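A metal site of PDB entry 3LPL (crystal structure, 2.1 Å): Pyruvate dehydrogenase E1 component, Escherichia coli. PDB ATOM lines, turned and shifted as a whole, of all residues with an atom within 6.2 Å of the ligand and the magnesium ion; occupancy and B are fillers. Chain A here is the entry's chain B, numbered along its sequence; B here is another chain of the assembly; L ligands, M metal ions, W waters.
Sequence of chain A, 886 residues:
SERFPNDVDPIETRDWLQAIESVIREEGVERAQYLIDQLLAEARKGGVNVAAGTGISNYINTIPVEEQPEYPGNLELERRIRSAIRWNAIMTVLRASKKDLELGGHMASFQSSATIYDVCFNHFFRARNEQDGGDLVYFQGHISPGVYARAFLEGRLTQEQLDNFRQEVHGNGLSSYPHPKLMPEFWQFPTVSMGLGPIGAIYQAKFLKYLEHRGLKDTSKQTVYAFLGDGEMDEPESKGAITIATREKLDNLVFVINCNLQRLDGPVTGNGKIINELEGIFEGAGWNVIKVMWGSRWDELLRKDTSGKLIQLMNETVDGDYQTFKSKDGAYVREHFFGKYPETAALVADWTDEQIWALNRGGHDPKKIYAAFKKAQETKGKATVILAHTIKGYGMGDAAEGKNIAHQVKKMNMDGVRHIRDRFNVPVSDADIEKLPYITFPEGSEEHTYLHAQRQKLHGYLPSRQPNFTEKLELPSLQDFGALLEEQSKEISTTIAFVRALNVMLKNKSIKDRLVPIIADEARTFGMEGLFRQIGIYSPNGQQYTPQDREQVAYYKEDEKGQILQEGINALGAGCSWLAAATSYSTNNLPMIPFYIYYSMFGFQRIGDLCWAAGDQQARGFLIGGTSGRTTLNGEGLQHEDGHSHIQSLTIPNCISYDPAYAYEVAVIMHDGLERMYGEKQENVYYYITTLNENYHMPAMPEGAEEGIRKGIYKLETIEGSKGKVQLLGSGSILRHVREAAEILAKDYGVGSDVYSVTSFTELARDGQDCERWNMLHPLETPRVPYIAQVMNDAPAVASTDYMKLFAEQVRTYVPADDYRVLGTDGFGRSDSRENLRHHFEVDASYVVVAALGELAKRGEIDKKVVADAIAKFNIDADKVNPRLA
Met 194 touches the ligand (CE to O2, 2.8 Å). Gly 229 touches the ligand (CA to O2, 3.3 Å). Asn 258 touches the ligand (ND2 to O6, 3.5 Å). Arg 263 touches the ligand (CA to O1, 3.8 Å). CB of Leu 264 touches C1 of the ligand, at 3.8 Å. CD1 of Ile 569 of chain B touches O1 of the ligand (3.5 Å). Hydrophobic or aromatic side chains that line the ligand: His 142, Met 194, Leu 264 and Ile 569 of chain B. Of the 24 residues printed, 15 come within 4 Å of the ligand. The nearest printed residue that does not touch the ligand is Asp 521 of chain B (4.3 Å).
The magnesium ion is bound by O3 of the ligand (2.1 Å), OD1 of Asp 230 (2.1 Å), O of Gln 262 (2.2 Å), water W2 (2.2 Å), OD1 of Asn 260 (2.3 Å) and O5 of the ligand (2.5 Å).
Water W2 lies within hydrogen-bond range of the backbone carbonyl oxygen of Asn 258, an oxygen (O6) of the ligand, the backbone NH of Asp 230 and the side-chain amide nitrogen of Asn 260. Water W3 lies within hydrogen-bond range of the side-chain amide nitrogen (NE2) of Gln 140, the side-chain carboxylate (OE1) of Glu 232, an oxygen (O2) of the ligand and the backbone NH (N) of Gly 229. Water W1 lies within hydrogen-bond range of the side-chain amide oxygen (OE1) of Gln 140 (2.5 Å), the side-chain hydroxyl (OG) of Ser 109 (2.6 Å), the side-chain amide nitrogen (ND2) of Asn 258 (2.8 Å) and an oxygen (O6) of the ligand (3.4 Å).
ND2 of Asn 258 sits at hydrogen-bond distance from OG of Ser 112. OD2 of Asp 521 of chain B sits at hydrogen-bond distance from N of Leu 264 (2.9 Å). The side-chain carboxylate of Glu 232 sits at hydrogen-bond distance from the backbone NH of Gly 229 (3.3 Å). The backbone NH of Asp 230 sits at hydrogen-bond distance from the backbone carbonyl oxygen of Asn 258 (3.3 Å). NE2 of Gln 140 lies close to N of Gly 229, 3.1 Å away. The backbone NH of Leu 261 lies within hydrogen-bond range of the side-chain carboxylate of Asp 230, at 2.7 Å. The side-chain amino group (NZ) of Lys 392 sits at hydrogen-bond distance from the backbone carbonyl oxygen (O) of Arg 263, 3.0 Å away. OG of Ser 109 lies within hydrogen-bond range of NE2 of His 142 (3.2 Å).
OG of Ser 109 is in hydrogen-bond range of O7 of the ligand, 3.1 Å away. The backbone NH (N) of Gly 231 lies close to an oxygen (O3) of the ligand, 2.9 Å away. NE2 of His 142 sits at hydrogen-bond distance from O7 of the ligand, at 2.4 Å. An oxygen (O4) of the ligand is in hydrogen-bond range of the side-chain amide nitrogen (NE2) of Gln 140 (3.3 Å). The backbone NH (N) of Glu 232 sits at hydrogen-bond distance from an oxygen (O2) of the ligand, at 2.8 Å. NZ of Lys 392 is in salt-bridge range of O7 of the ligand.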
ATOM      1  N   ALA A 108      -6.303 -11.492   6.624  1.00  0.00           N
ATOM      2  CA  ALA A 108      -5.326 -10.688   5.899  1.00  0.00           C
ATOM      3  C   ALA A 108      -5.918  -9.931   4.720  1.00  0.00           C
ATOM      4  O   ALA A 108      -5.657  -8.735   4.549  1.00  0.00           O
ATOM      5  CB  ALA A 108      -4.167 -11.578   5.418  1.00  0.00           C
ATOM      6  N   SER A 109      -6.759 -10.585   3.923  1.00  0.00           N
ATOM      7  CA  SER A 109      -7.342  -9.890   2.765  1.00  0.00           C
ATOM      8  C   SER A 109      -8.242  -8.675   3.103  1.00  0.00           C
ATOM      9  O   SER A 109      -8.021  -7.574   2.566  1.00  0.00           O
ATOM     10  CB  SER A 109      -8.096 -10.875   1.881  1.00  0.00           C
ATOM     11  OG  SER A 109      -8.595 -10.217   0.720  1.00  0.00           O
ATOM     12  N   SER A 112      -6.356  -5.641   4.078  1.00  0.00           N
ATOM     13  CA  SER A 112      -5.695  -4.882   3.047  1.00  0.00           C
ATOM     14  C   SER A 112      -6.656  -4.005   2.243  1.00  0.00           C
ATOM     15  O   SER A 112      -6.266  -2.945   1.757  1.00  0.00           O
ATOM     16  CB  SER A 112      -4.921  -5.811   2.101  1.00  0.00           C
ATOM     17  OG  SER A 112      -5.752  -6.478   1.175  1.00  0.00           O
ATOM     18  N   GLN A 140     -15.504  -9.209  -3.111  1.00  0.00           N
ATOM     19  CA  GLN A 140     -14.503 -10.248  -3.208  1.00  0.00           C
ATOM     20  C   GLN A 140     -14.920 -11.231  -2.110  1.00  0.00           C
ATOM     21  O   GLN A 140     -15.150 -10.849  -0.961  1.00  0.00           O
ATOM     22  CB  GLN A 140     -13.124  -9.658  -2.951  1.00  0.00           C
ATOM     23  CG  GLN A 140     -11.975 -10.625  -3.099  1.00  0.00           C
ATOM     24  CD  GLN A 140     -10.652  -9.890  -2.974  1.00  0.00           C
ATOM     25  OE1 GLN A 140     -10.506  -9.000  -2.124  1.00  0.00           O
ATOM     26  NE2 GLN A 140      -9.685 -10.234  -3.831  1.00  0.00           N
ATOM     27  N   HIS A 142     -13.593 -13.747  -0.120  1.00  0.00           N
ATOM     28  CA  HIS A 142     -12.973 -13.986   1.174  1.00  0.00           C
ATOM     29  C   HIS A 142     -12.887 -12.791   2.113  1.00  0.00           C
ATOM     30  O   HIS A 142     -12.297 -12.902   3.169  1.00  0.00           O
ATOM     31  CB  HIS A 142     -11.594 -14.669   0.992  1.00  0.00           C
ATOM     32  CG  HIS A 142     -10.678 -13.979   0.047  1.00  0.00           C
ATOM     33  ND1 HIS A 142     -10.985 -13.794  -1.295  1.00  0.00           N
ATOM     34  CD2 HIS A 142      -9.455 -13.423   0.221  1.00  0.00           C
ATOM     35  CE1 HIS A 142      -9.990 -13.160  -1.889  1.00  0.00           C
ATOM     36  NE2 HIS A 142      -9.051 -12.917  -0.995  1.00  0.00           N
ATOM     37  N   ILE A 143     -13.498 -11.661   1.747  1.00  0.00           N
ATOM     38  CA  ILE A 143     -13.493 -10.541   2.691  1.00  0.00           C
ATOM     39  C   ILE A 143     -14.850 -10.461   3.389  1.00  0.00           C
ATOM     40  O   ILE A 143     -15.135  -9.497   4.101  1.00  0.00           O
ATOM     41  CB  ILE A 143     -13.101  -9.172   2.024  1.00  0.00           C
ATOM     42  CG1 ILE A 143     -14.002  -8.802   0.841  1.00  0.00           C
ATOM     43  CG2 ILE A 143     -11.654  -9.265   1.494  1.00  0.00           C
ATOM     44  CD1 ILE A 143     -15.426  -8.428   1.221  1.00  0.00           C
ATOM     45  N   MET A 194     -13.136 -17.781  -8.046  1.00  0.00           N
ATOM     46  CA  MET A 194     -12.448 -16.737  -8.745  1.00  0.00           C
ATOM     47  C   MET A 194     -12.533 -16.763 -10.245  1.00  0.00           C
ATOM     48  O   MET A 194     -12.652 -17.825 -10.862  1.00  0.00           O
ATOM     49  CB  MET A 194     -10.996 -16.676  -8.259  1.00  0.00           C
ATOM     50  CG  MET A 194     -10.923 -15.963  -6.881  1.00  0.00           C
ATOM     51  SD  MET A 194      -9.528 -16.433  -5.899  1.00  0.00           S
ATOM     52  CE  MET A 194      -8.463 -15.116  -6.185  1.00  0.00           C
ATOM     53  N   LEU A 228     -12.042  -7.322  -7.156  1.00  0.00           N
ATOM     54  CA  LEU A 228     -11.191  -8.452  -7.495  1.00  0.00           C
ATOM     55  C   LEU A 228      -9.804  -8.411  -6.872  1.00  0.00           C
ATOM     56  O   LEU A 228      -9.311  -7.340  -6.491  1.00  0.00           O
ATOM     57  CB  LEU A 228     -11.019  -8.481  -9.021  1.00  0.00           C
ATOM     58  CG  LEU A 228     -12.258  -8.078  -9.840  1.00  0.00           C
ATOM     59  CD1 LEU A 228     -11.824  -7.670 -11.238  1.00  0.00           C
ATOM     60  CD2 LEU A 228     -13.247  -9.233  -9.868  1.00  0.00           C
ATOM     61  N   GLY A 229      -9.178  -9.597  -6.780  1.00  0.00           N
ATOM     62  CA  GLY A 229      -7.838  -9.695  -6.245  1.00  0.00           C
ATOM     63  C   GLY A 229      -6.885  -9.607  -7.436  1.00  0.00           C
ATOM     64  O   GLY A 229      -7.302  -9.843  -8.579  1.00  0.00           O
ATOM     65  N   ASP A 230      -5.616  -9.244  -7.215  1.00  0.00           N
ATOM     66  CA  ASP A 230      -4.727  -9.184  -8.366  1.00  0.00           C
ATOM     67  C   ASP A 230      -4.365 -10.607  -8.792  1.00  0.00           C
ATOM     68  O   ASP A 230      -4.278 -10.911  -9.979  1.00  0.00           O
ATOM     69  CB  ASP A 230      -3.482  -8.315  -8.131  1.00  0.00           C
ATOM     70  CG  ASP A 230      -2.830  -8.546  -6.772  1.00  0.00           C
ATOM     71  OD1 ASP A 230      -3.222  -9.445  -6.040  1.00  0.00           O
ATOM     72  OD2 ASP A 230      -1.896  -7.795  -6.458  1.00  0.00           O
ATOM     73  N   GLY A 231      -4.188 -11.494  -7.819  1.00  0.00           N
ATOM     74  CA  GLY A 231      -3.880 -12.875  -8.141  1.00  0.00           C
ATOM     75  C   GLY A 231      -4.996 -13.480  -8.989  1.00  0.00           C
ATOM     76  O   GLY A 231      -4.733 -14.207  -9.950  1.00  0.00           O
ATOM     77  N   GLU A 232      -6.247 -13.169  -8.639  1.00  0.00           N
ATOM     78  CA  GLU A 232      -7.430 -13.644  -9.360  1.00  0.00           C
ATOM     79  C   GLU A 232      -7.423 -13.288 -10.858  1.00  0.00           C
ATOM     80  O   GLU A 232      -8.036 -13.993 -11.669  1.00  0.00           O
ATOM     81  CB  GLU A 232      -8.703 -13.069  -8.697  1.00  0.00           C
ATOM     82  CG  GLU A 232      -9.989 -13.302  -9.491  1.00  0.00           C
ATOM     83  CD  GLU A 232     -11.256 -12.844  -8.755  1.00  0.00           C
ATOM     84  OE1 GLU A 232     -11.153 -12.051  -7.784  1.00  0.00           O
ATOM     85  OE2 GLU A 232     -12.361 -13.256  -9.166  1.00  0.00           O
ATOM     86  N   MET A 233      -6.760 -12.195 -11.217  1.00  0.00           N
ATOM     87  CA  MET A 233      -6.688 -11.788 -12.617  1.00  0.00           C
ATOM     88  C   MET A 233      -5.968 -12.779 -13.538  1.00  0.00           C
ATOM     89  O   MET A 233      -6.018 -12.639 -14.767  1.00  0.00           O
ATOM     90  CB  MET A 233      -6.032 -10.405 -12.742  1.00  0.00           C
ATOM     91  CG  MET A 233      -6.711  -9.286 -11.936  1.00  0.00           C
ATOM     92  SD  MET A 233      -8.541  -9.254 -12.046  1.00  0.00           S
ATOM     93  CE  MET A 233      -8.730  -9.002 -13.856  1.00  0.00           C
ATOM     94  N   ASN A 258      -7.660  -5.059  -6.161  1.00  0.00           N
ATOM     95  CA  ASN A 258      -6.851  -4.891  -4.962  1.00  0.00           C
ATOM     96  C   ASN A 258      -5.432  -5.380  -5.284  1.00  0.00           C
ATOM     97  O   ASN A 258      -5.154  -6.571  -5.313  1.00  0.00           O
ATOM     98  CB  ASN A 258      -7.443  -5.688  -3.802  1.00  0.00           C
ATOM     99  CG  ASN A 258      -6.668  -5.473  -2.525  1.00  0.00           C
ATOM    100  OD1 ASN A 258      -5.849  -4.554  -2.446  1.00  0.00           O
ATOM    101  ND2 ASN A 258      -6.925  -6.286  -1.517  1.00  0.00           N
ATOM    102  N   CYS A 259      -4.551  -4.427  -5.557  1.00  0.00           N
ATOM    103  CA  CYS A 259      -3.189  -4.769  -5.901  1.00  0.00           C
ATOM    104  C   CYS A 259      -2.249  -4.783  -4.698  1.00  0.00           C
ATOM    105  O   CYS A 259      -1.487  -3.827  -4.479  1.00  0.00           O
ATOM    106  CB  CYS A 259      -2.682  -3.808  -6.978  1.00  0.00           C
ATOM    107  SG  CYS A 259      -3.634  -3.915  -8.545  1.00  0.00           S
ATOM    108  N   ASN A 260      -2.317  -5.852  -3.907  1.00  0.00           N
ATOM    109  CA  ASN A 260      -1.426  -5.973  -2.762  1.00  0.00           C
ATOM    110  C   ASN A 260      -0.171  -6.743  -3.202  1.00  0.00           C
ATOM    111  O   ASN A 260       0.728  -6.982  -2.409  1.00  0.00           O
ATOM    112  CB  ASN A 260      -2.111  -6.651  -1.556  1.00  0.00           C
ATOM    113  CG  ASN A 260      -2.868  -7.928  -1.929  1.00  0.00           C
ATOM    114  OD1 ASN A 260      -2.453  -8.672  -2.800  1.00  0.00           O
ATOM    115  ND2 ASN A 260      -3.970  -8.187  -1.237  1.00  0.00           N
ATOM    116  N   LEU A 261      -0.128  -7.106  -4.479  1.00  0.00           N
ATOM    117  CA  LEU A 261       1.001  -7.792  -5.100  1.00  0.00           C
ATOM    118  C   LEU A 261       1.193  -9.257  -4.766  1.00  0.00           C
ATOM    119  O   LEU A 261       2.213  -9.856  -5.131  1.00  0.00           O
ATOM    120  CB  LEU A 261       2.307  -7.059  -4.783  1.00  0.00           C
ATOM    121  CG  LEU A 261       2.317  -5.551  -4.991  1.00  0.00           C
ATOM    122  CD1 LEU A 261       3.727  -5.045  -4.695  1.00  0.00           C
ATOM    123  CD2 LEU A 261       1.891  -5.202  -6.420  1.00  0.00           C
ATOM    124  N   GLN A 262       0.229  -9.851  -4.076  1.00  0.00           N
ATOM    125  CA  GLN A 262       0.418 -11.241  -3.763  1.00  0.00           C
ATOM    126  C   GLN A 262      -0.816 -12.106  -3.883  1.00  0.00           C
ATOM    127  O   GLN A 262      -1.934 -11.636  -3.705  1.00  0.00           O
ATOM    128  CB  GLN A 262       1.013 -11.388  -2.352  1.00  0.00           C
ATOM    129  CG  GLN A 262       0.103 -10.941  -1.249  1.00  0.00           C
ATOM    130  CD  GLN A 262       0.817 -10.894   0.090  1.00  0.00           C
ATOM    131  OE1 GLN A 262       1.622  -9.988   0.358  1.00  0.00           O
ATOM    132  NE2 GLN A 262       0.531 -11.882   0.943  1.00  0.00           N
ATOM    133  N   ARG A 263      -0.599 -13.365  -4.222  1.00  0.00           N
ATOM    134  CA  ARG A 263      -1.690 -14.324  -4.320  1.00  0.00           C
ATOM    135  C   ARG A 263      -1.657 -14.917  -2.900  1.00  0.00           C
ATOM    136  O   ARG A 263      -1.319 -14.225  -1.956  1.00  0.00           O
ATOM    137  CB  ARG A 263      -1.385 -15.424  -5.358  1.00  0.00           C
ATOM    138  CG  ARG A 263      -0.665 -14.997  -6.641  1.00  0.00           C
ATOM    139  CD  ARG A 263      -0.266 -16.249  -7.439  1.00  0.00           C
ATOM    140  NE  ARG A 263       0.415 -17.115  -6.507  1.00  0.00           N
ATOM    141  CZ  ARG A 263       1.679 -17.496  -6.611  1.00  0.00           C
ATOM    142  NH1 ARG A 263       2.411 -17.108  -7.641  1.00  0.00           N
ATOM    143  NH2 ARG A 263       2.242 -18.172  -5.605  1.00  0.00           N
ATOM    144  N   LEU A 264      -1.969 -16.210  -2.758  1.00  0.00           N
ATOM    145  CA  LEU A 264      -1.960 -16.840  -1.437  1.00  0.00           C
ATOM    146  C   LEU A 264      -0.532 -17.307  -1.094  1.00  0.00           C
ATOM    147  O   LEU A 264      -0.022 -17.018  -0.004  1.00  0.00           O
ATOM    148  CB  LEU A 264      -2.906 -18.046  -1.442  1.00  0.00           C
ATOM    149  CG  LEU A 264      -3.249 -18.809  -0.150  1.00  0.00           C
ATOM    150  CD1 LEU A 264      -4.704 -19.343  -0.215  1.00  0.00           C
ATOM    151  CD2 LEU A 264      -2.251 -19.962   0.039  1.00  0.00           C
ATOM    152  N   VAL A 268       2.336 -12.186  -6.904  1.00  0.00           N
ATOM    153  CA  VAL A 268       1.718 -12.548  -8.189  1.00  0.00           C
ATOM    154  C   VAL A 268       2.772 -12.708  -9.293  1.00  0.00           C
ATOM    155  O   VAL A 268       2.712 -13.632 -10.096  1.00  0.00           O
ATOM    156  CB  VAL A 268       0.641 -11.526  -8.602  1.00  0.00           C
ATOM    157  CG1 VAL A 268      -0.082 -11.992  -9.858  1.00  0.00           C
ATOM    158  CG2 VAL A 268      -0.365 -11.367  -7.482  1.00  0.00           C
ATOM    159  N   LYS A 392      -1.015  -6.443   2.028  1.00  0.00           N
ATOM    160  CA  LYS A 392      -1.800  -7.563   2.549  1.00  0.00           C
ATOM    161  C   LYS A 392      -1.352  -7.882   3.981  1.00  0.00           C
ATOM    162  O   LYS A 392      -0.139  -7.952   4.277  1.00  0.00           O
ATOM    163  CB  LYS A 392      -1.643  -8.810   1.670  1.00  0.00           C
ATOM    164  CG  LYS A 392      -2.686  -9.893   1.956  1.00  0.00           C
ATOM    165  CD  LYS A 392      -2.583 -10.993   0.883  1.00  0.00           C
ATOM    166  CE  LYS A 392      -3.623 -12.108   1.053  1.00  0.00           C
ATOM    167  NZ  LYS A 392      -3.431 -13.114  -0.065  1.00  0.00           N
ATOM    168  N   ASP B 521      -1.340 -22.024  -7.393  1.00  0.00           N
ATOM    169  CA  ASP B 521      -1.092 -21.141  -6.237  1.00  0.00           C
ATOM    170  C   ASP B 521      -0.919 -21.953  -4.970  1.00  0.00           C
ATOM    171  O   ASP B 521       0.196 -22.115  -4.441  1.00  0.00           O
ATOM    172  CB  ASP B 521      -2.223 -20.103  -6.053  1.00  0.00           C
ATOM    173  CG  ASP B 521      -1.865 -18.983  -5.029  1.00  0.00           C
ATOM    174  OD1 ASP B 521      -0.648 -18.698  -4.798  1.00  0.00           O
ATOM    175  OD2 ASP B 521      -2.808 -18.346  -4.491  1.00  0.00           O
ATOM    176  N   ILE B 569      -3.341 -18.565  -9.531  1.00  0.00           N
ATOM    177  CA  ILE B 569      -4.788 -18.811  -9.517  1.00  0.00           C
ATOM    178  C   ILE B 569      -5.249 -18.909 -10.960  1.00  0.00           C
ATOM    179  O   ILE B 569      -5.738 -17.951 -11.557  1.00  0.00           O
ATOM    180  CB  ILE B 569      -5.512 -17.667  -8.787  1.00  0.00           C
ATOM    181  CG1 ILE B 569      -4.944 -17.525  -7.359  1.00  0.00           C
ATOM    182  CG2 ILE B 569      -6.994 -17.943  -8.755  1.00  0.00           C
ATOM    183  CD1 ILE B 569      -5.253 -16.216  -6.684  1.00  0.00           C
HETATM  184  C1  LIG L   1      -5.871 -15.965  -2.703  1.00  0.00           C
HETATM  185  C2  LIG L   1      -6.486 -14.726  -3.351  1.00  0.00           C
HETATM  186  O1  LIG L   1      -5.500 -13.929  -4.023  1.00  0.00           O
HETATM  187  P1  LIG L   1      -5.927 -12.541  -4.711  1.00  0.00           P
HETATM  188  O2  LIG L   1      -6.791 -12.830  -5.881  1.00  0.00           O
HETATM  189  O3  LIG L   1      -4.690 -11.755  -4.933  1.00  0.00           O
HETATM  190  O4  LIG L   1      -6.837 -11.864  -3.558  1.00  0.00           O
HETATM  191  P2  LIG L   1      -6.230 -11.201  -2.216  1.00  0.00           P
HETATM  192  O5  LIG L   1      -4.638 -11.464  -2.215  1.00  0.00           O
HETATM  193  O6  LIG L   1      -6.575  -9.763  -2.127  1.00  0.00           O
HETATM  194  O7  LIG L   1      -6.813 -12.040  -0.971  1.00  0.00           O
HETATM  195 MG    MG M   1      -3.584 -10.190  -4.067  1.00  0.00          MG
HETATM  196  O   HOH W   1      -8.909  -7.948  -0.529  1.00  0.00           O
HETATM  197  O   HOH W   2      -5.280  -8.723  -4.176  1.00  0.00           O
HETATM  198  O   HOH W   3      -9.675 -12.553  -5.273  1.00  0.00           O
